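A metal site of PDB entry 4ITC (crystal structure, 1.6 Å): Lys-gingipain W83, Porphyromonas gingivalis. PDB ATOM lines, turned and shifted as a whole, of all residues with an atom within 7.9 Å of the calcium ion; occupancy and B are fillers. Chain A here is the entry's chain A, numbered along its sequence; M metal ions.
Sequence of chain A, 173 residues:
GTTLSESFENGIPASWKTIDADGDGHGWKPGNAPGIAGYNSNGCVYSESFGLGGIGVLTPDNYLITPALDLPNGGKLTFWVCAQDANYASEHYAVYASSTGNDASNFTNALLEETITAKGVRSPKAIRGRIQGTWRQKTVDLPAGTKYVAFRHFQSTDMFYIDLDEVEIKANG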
ATOM      1  N   GLU A   6      21.280  -2.270 -27.181  1.00  0.00           N
ATOM      2  CA  GLU A   6      22.267  -2.559 -26.157  1.00  0.00           C
ATOM      3  C   GLU A   6      22.795  -1.293 -25.536  1.00  0.00           C
ATOM      4  O   GLU A   6      23.386  -0.434 -26.200  1.00  0.00           O
ATOM      5  CB  GLU A   6      23.406  -3.417 -26.659  1.00  0.00           C
ATOM      6  CG  GLU A   6      24.440  -3.747 -25.575  1.00  0.00           C
ATOM      7  CD  GLU A   6      23.838  -4.407 -24.331  1.00  0.00           C
ATOM      8  OE1 GLU A   6      23.191  -5.472 -24.511  1.00  0.00           O
ATOM      9  OE2 GLU A   6      24.000  -3.909 -23.180  1.00  0.00           O
ATOM     10  N   SER A   7      22.520  -1.159 -24.223  1.00  0.00           N
ATOM     11  CA  SER A   7      22.886   0.010 -23.471  1.00  0.00           C
ATOM     12  C   SER A   7      24.190  -0.104 -22.705  1.00  0.00           C
ATOM     13  O   SER A   7      24.692   0.875 -22.137  1.00  0.00           O
ATOM     14  CB  SER A   7      21.754   0.388 -22.503  1.00  0.00           C
ATOM     15  OG  SER A   7      20.597   0.814 -23.210  1.00  0.00           O
ATOM     16  N   PHE A   8      24.768  -1.291 -22.672  1.00  0.00           N
ATOM     17  CA  PHE A   8      26.011  -1.540 -21.967  1.00  0.00           C
ATOM     18  C   PHE A   8      26.025  -1.127 -20.482  1.00  0.00           C
ATOM     19  O   PHE A   8      27.046  -0.694 -19.953  1.00  0.00           O
ATOM     20  CB  PHE A   8      27.191  -0.872 -22.711  1.00  0.00           C
ATOM     21  CG  PHE A   8      27.367  -1.374 -24.102  1.00  0.00           C
ATOM     22  CD1 PHE A   8      27.806  -2.661 -24.344  1.00  0.00           C
ATOM     23  CD2 PHE A   8      27.123  -0.540 -25.182  1.00  0.00           C
ATOM     24  CE1 PHE A   8      27.966  -3.161 -25.651  1.00  0.00           C
ATOM     25  CE2 PHE A   8      27.271  -1.032 -26.459  1.00  0.00           C
ATOM     26  CZ  PHE A   8      27.675  -2.326 -26.697  1.00  0.00           C
ATOM     27  N   GLU A   9      24.898  -1.289 -19.820  1.00  0.00           N
ATOM     28  CA  GLU A   9      24.807  -0.885 -18.418  1.00  0.00           C
ATOM     29  C   GLU A   9      25.457  -1.918 -17.518  1.00  0.00           C
ATOM     30  O   GLU A   9      25.817  -1.608 -16.370  1.00  0.00           O
ATOM     31  CB  GLU A   9      23.339  -0.612 -18.022  1.00  0.00           C
ATOM     32  CG  GLU A   9      22.726   0.542 -18.803  1.00  0.00           C
ATOM     33  CD  GLU A   9      23.552   1.803 -18.721  1.00  0.00           C
ATOM     34  OE1 GLU A   9      23.897   2.224 -17.592  1.00  0.00           O
ATOM     35  OE2 GLU A   9      23.855   2.426 -19.768  1.00  0.00           O
ATOM     36  N   ASN A  10      25.604  -3.139 -18.009  1.00  0.00           N
ATOM     37  CA  ASN A  10      26.278  -4.210 -17.277  1.00  0.00           C
ATOM     38  C   ASN A  10      27.340  -4.895 -18.103  1.00  0.00           C
ATOM     39  O   ASN A  10      27.453  -6.116 -18.144  1.00  0.00           O
ATOM     40  CB  ASN A  10      25.225  -5.180 -16.728  1.00  0.00           C
ATOM     41  CG  ASN A  10      24.407  -4.549 -15.632  1.00  0.00           C
ATOM     42  OD1 ASN A  10      23.262  -4.149 -15.823  1.00  0.00           O
ATOM     43  ND2 ASN A  10      25.034  -4.390 -14.511  1.00  0.00           N
ATOM     44  N   GLY A  31      32.980   0.487 -19.565  1.00  0.00           N
ATOM     45  CA  GLY A  31      33.239   1.690 -18.815  1.00  0.00           C
ATOM     46  C   GLY A  31      31.995   2.043 -18.040  1.00  0.00           C
ATOM     47  O   GLY A  31      30.881   1.765 -18.481  1.00  0.00           O
ATOM     48  N   ALA A  37      31.436   7.632 -17.866  1.00  0.00           N
ATOM     49  CA  ALA A  37      29.986   7.639 -17.928  1.00  0.00           C
ATOM     50  C   ALA A  37      29.523   7.413 -19.352  1.00  0.00           C
ATOM     51  O   ALA A  37      30.116   7.925 -20.284  1.00  0.00           O
ATOM     52  CB  ALA A  37      29.450   8.980 -17.434  1.00  0.00           C
ATOM     53  N   GLY A  38      28.413   6.720 -19.491  1.00  0.00           N
ATOM     54  CA  GLY A  38      27.761   6.587 -20.783  1.00  0.00           C
ATOM     55  C   GLY A  38      26.930   7.776 -21.216  1.00  0.00           C
ATOM     56  O   GLY A  38      26.897   8.864 -20.602  1.00  0.00           O
ATOM     57  N   TYR A  39      26.308   7.616 -22.368  1.00  0.00           N
ATOM     58  CA  TYR A  39      25.407   8.641 -22.885  1.00  0.00           C
ATOM     59  C   TYR A  39      24.080   8.536 -22.143  1.00  0.00           C
ATOM     60  O   TYR A  39      23.398   7.531 -22.212  1.00  0.00           O
ATOM     61  CB  TYR A  39      25.215   8.505 -24.395  1.00  0.00           C
ATOM     62  CG  TYR A  39      24.170   9.497 -24.841  1.00  0.00           C
ATOM     63  CD1 TYR A  39      24.445  10.848 -24.852  1.00  0.00           C
ATOM     64  CD2 TYR A  39      22.908   9.062 -25.156  1.00  0.00           C
ATOM     65  CE1 TYR A  39      23.458  11.770 -25.157  1.00  0.00           C
ATOM     66  CE2 TYR A  39      21.926   9.982 -25.493  1.00  0.00           C
ATOM     67  CZ  TYR A  39      22.236  11.313 -25.500  1.00  0.00           C
ATOM     68  OH  TYR A  39      21.240  12.203 -25.838  1.00  0.00           O
ATOM     69  N   ASN A  40      23.751   9.588 -21.405  1.00  0.00           N
ATOM     70  CA  ASN A  40      22.497   9.637 -20.639  1.00  0.00           C
ATOM     71  C   ASN A  40      22.266   8.360 -19.861  1.00  0.00           C
ATOM     72  O   ASN A  40      21.144   7.865 -19.763  1.00  0.00           O
ATOM     73  CB  ASN A  40      21.332   9.975 -21.581  1.00  0.00           C
ATOM     74  CG  ASN A  40      20.013  10.258 -20.844  1.00  0.00           C
ATOM     75  OD1 ASN A  40      18.900  10.003 -21.385  1.00  0.00           O
ATOM     76  ND2 ASN A  40      20.116  10.763 -19.639  1.00  0.00           N
ATOM     77  N   SER A  41      23.341   7.815 -19.313  1.00  0.00           N
ATOM     78  CA  SER A  41      23.356   6.502 -18.677  1.00  0.00           C
ATOM     79  C   SER A  41      24.709   6.258 -18.012  1.00  0.00           C
ATOM     80  O   SER A  41      25.650   6.931 -18.304  1.00  0.00           O
ATOM     81  CB  SER A  41      23.037   5.418 -19.685  1.00  0.00           C
ATOM     82  OG  SER A  41      24.056   5.268 -20.668  1.00  0.00           O
ATOM     83  N   ASN A  42      24.751   5.200 -17.200  1.00  0.00           N
ATOM     84  CA  ASN A  42      25.857   4.862 -16.305  1.00  0.00           C
ATOM     85  C   ASN A  42      27.022   4.088 -16.958  1.00  0.00           C
ATOM     86  O   ASN A  42      28.173   4.116 -16.491  1.00  0.00           O
ATOM     87  CB  ASN A  42      25.259   3.987 -15.199  1.00  0.00           C
ATOM     88  CG  ASN A  42      26.160   3.869 -13.978  1.00  0.00           C
ATOM     89  OD1 ASN A  42      26.442   4.871 -13.319  1.00  0.00           O
ATOM     90  ND2 ASN A  42      26.560   2.650 -13.633  1.00  0.00           N
ATOM     91  N   GLY A  43      26.690   3.324 -17.971  1.00  0.00           N
ATOM     92  CA  GLY A  43      27.616   2.390 -18.604  1.00  0.00           C
ATOM     93  C   GLY A  43      27.781   2.587 -20.095  1.00  0.00           C
ATOM     94  O   GLY A  43      26.895   3.066 -20.784  1.00  0.00           O
ATOM     95  N   CYS A  44      28.982   2.268 -20.565  1.00  0.00           N
ATOM     96  CA  CYS A  44      29.285   2.312 -22.002  1.00  0.00           C
ATOM     97  C   CYS A  44      30.439   1.372 -22.274  1.00  0.00           C
ATOM     98  O   CYS A  44      30.790   0.575 -21.409  1.00  0.00           O
ATOM     99  CB  CYS A  44      29.623   3.713 -22.447  1.00  0.00           C
ATOM    100  SG  CYS A  44      31.144   4.416 -21.787  1.00  0.00           S
ATOM    101  N   VAL A  45      30.990   1.413 -23.498  1.00  0.00           N
ATOM    102  CA  VAL A  45      32.229   0.717 -23.792  1.00  0.00           C
ATOM    103  C   VAL A  45      33.240   1.707 -24.323  1.00  0.00           C
ATOM    104  O   VAL A  45      32.900   2.766 -24.825  1.00  0.00           O
ATOM    105  CB  VAL A  45      32.030  -0.434 -24.810  1.00  0.00           C
ATOM    106  CG1 VAL A  45      31.123  -1.487 -24.196  1.00  0.00           C
ATOM    107  CG2 VAL A  45      31.472   0.070 -26.110  1.00  0.00           C
ATOM    108  N   TRP A 135      29.095  13.853 -26.656  1.00  0.00           N
ATOM    109  CA  TRP A 135      28.457  12.709 -27.334  1.00  0.00           C
ATOM    110  C   TRP A 135      27.766  13.139 -28.604  1.00  0.00           C
ATOM    111  O   TRP A 135      26.999  14.121 -28.598  1.00  0.00           O
ATOM    112  CB  TRP A 135      27.465  12.024 -26.422  1.00  0.00           C
ATOM    113  CG  TRP A 135      28.054  11.259 -25.269  1.00  0.00           C
ATOM    114  CD1 TRP A 135      28.171  11.673 -23.947  1.00  0.00           C
ATOM    115  CD2 TRP A 135      28.585   9.920 -25.306  1.00  0.00           C
ATOM    116  NE1 TRP A 135      28.733  10.691 -23.200  1.00  0.00           N
ATOM    117  CE2 TRP A 135      29.023   9.600 -23.997  1.00  0.00           C
ATOM    118  CE3 TRP A 135      28.748   8.959 -26.318  1.00  0.00           C
ATOM    119  CZ2 TRP A 135      29.599   8.370 -23.672  1.00  0.00           C
ATOM    120  CZ3 TRP A 135      29.338   7.729 -25.993  1.00  0.00           C
ATOM    121  CH2 TRP A 135      29.722   7.444 -24.659  1.00  0.00           C
ATOM    122  N   LEU A 164      31.737   4.454 -26.800  1.00  0.00           N
ATOM    123  CA  LEU A 164      30.645   4.027 -27.648  1.00  0.00           C
ATOM    124  C   LEU A 164      29.498   3.588 -26.742  1.00  0.00           C
ATOM    125  O   LEU A 164      29.724   2.912 -25.725  1.00  0.00           O
ATOM    126  CB  LEU A 164      31.092   2.847 -28.535  1.00  0.00           C
ATOM    127  CG  LEU A 164      30.018   2.077 -29.299  1.00  0.00           C
ATOM    128  CD1 LEU A 164      29.570   2.928 -30.464  1.00  0.00           C
ATOM    129  CD2 LEU A 164      30.558   0.745 -29.837  1.00  0.00           C
ATOM    130  N   ASP A 165      28.264   3.994 -27.095  1.00  0.00           N
ATOM    131  CA  ASP A 165      27.099   3.653 -26.256  1.00  0.00           C
ATOM    132  C   ASP A 165      25.820   3.566 -27.062  1.00  0.00           C
ATOM    133  O   ASP A 165      25.727   4.078 -28.198  1.00  0.00           O
ATOM    134  CB  ASP A 165      26.944   4.680 -25.118  1.00  0.00           C
ATOM    135  CG  ASP A 165      26.206   4.133 -23.907  1.00  0.00           C
ATOM    136  OD1 ASP A 165      25.945   2.916 -23.810  1.00  0.00           O
ATOM    137  OD2 ASP A 165      25.908   4.949 -22.991  1.00  0.00           O
ATOM    138  N   GLU A 166      24.843   2.875 -26.461  1.00  0.00           N
ATOM    139  CA  GLU A 166      23.436   2.931 -26.851  1.00  0.00           C
ATOM    140  C   GLU A 166      23.274   2.541 -28.323  1.00  0.00           C
ATOM    141  O   GLU A 166      22.834   3.342 -29.142  1.00  0.00           O
ATOM    142  CB  GLU A 166      22.880   4.299 -26.551  1.00  0.00           C
ATOM    143  CG  GLU A 166      22.945   4.637 -25.047  1.00  0.00           C
ATOM    144  CD  GLU A 166      22.243   3.672 -24.128  1.00  0.00           C
ATOM    145  OE1 GLU A 166      22.790   3.500 -23.003  1.00  0.00           O
ATOM    146  OE2 GLU A 166      21.199   3.064 -24.544  1.00  0.00           O
ATOM    147  N   VAL A 167      23.626   1.315 -28.608  1.00  0.00           N
ATOM    148  CA  VAL A 167      23.569   0.766 -29.970  1.00  0.00           C
ATOM    149  C   VAL A 167      22.184   0.220 -30.204  1.00  0.00           C
ATOM    150  O   VAL A 167      21.706  -0.589 -29.447  1.00  0.00           O
ATOM    151  CB  VAL A 167      24.573  -0.370 -30.146  1.00  0.00           C
ATOM    152  CG1 VAL A 167      24.375  -1.065 -31.500  1.00  0.00           C
ATOM    153  CG2 VAL A 167      25.989   0.175 -29.998  1.00  0.00           C
HETATM  154 CA    CA M   1      24.766   3.177 -21.703  1.00  0.00          CA
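N of Tyr 39 sits close to OD2 of Asp 165 (2.8 Å). N of Asn 42 sits at hydrogen-bond distance from OE1 of Glu 9 (3.1 Å). The backbone carbonyl oxygen (O) of Tyr 39 sits close to the side-chain hydroxyl (OG) of Ser 41, 2.8 Å away.
Six residues have an atom within 4 Å of the calcium ion: Ser 7, Glu 9, Ser 41, Gly 43, Asp 165 and Glu 166. The nearest printed residue that does not touch the calcium ion is Cys 44 (4.5 Å).
The calcium ion is bound by OE2 of Glu 9 (2.3 Å), O of Gly 43 (2.3 Å), O of Ser 7 (2.3 Å), OE1 of Glu 166 (2.4 Å), OD1 of Asp 165 (2.4 Å), OG of Ser 41 (2.4 Å) and OD2 of Asp 165 (2.5 Å).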
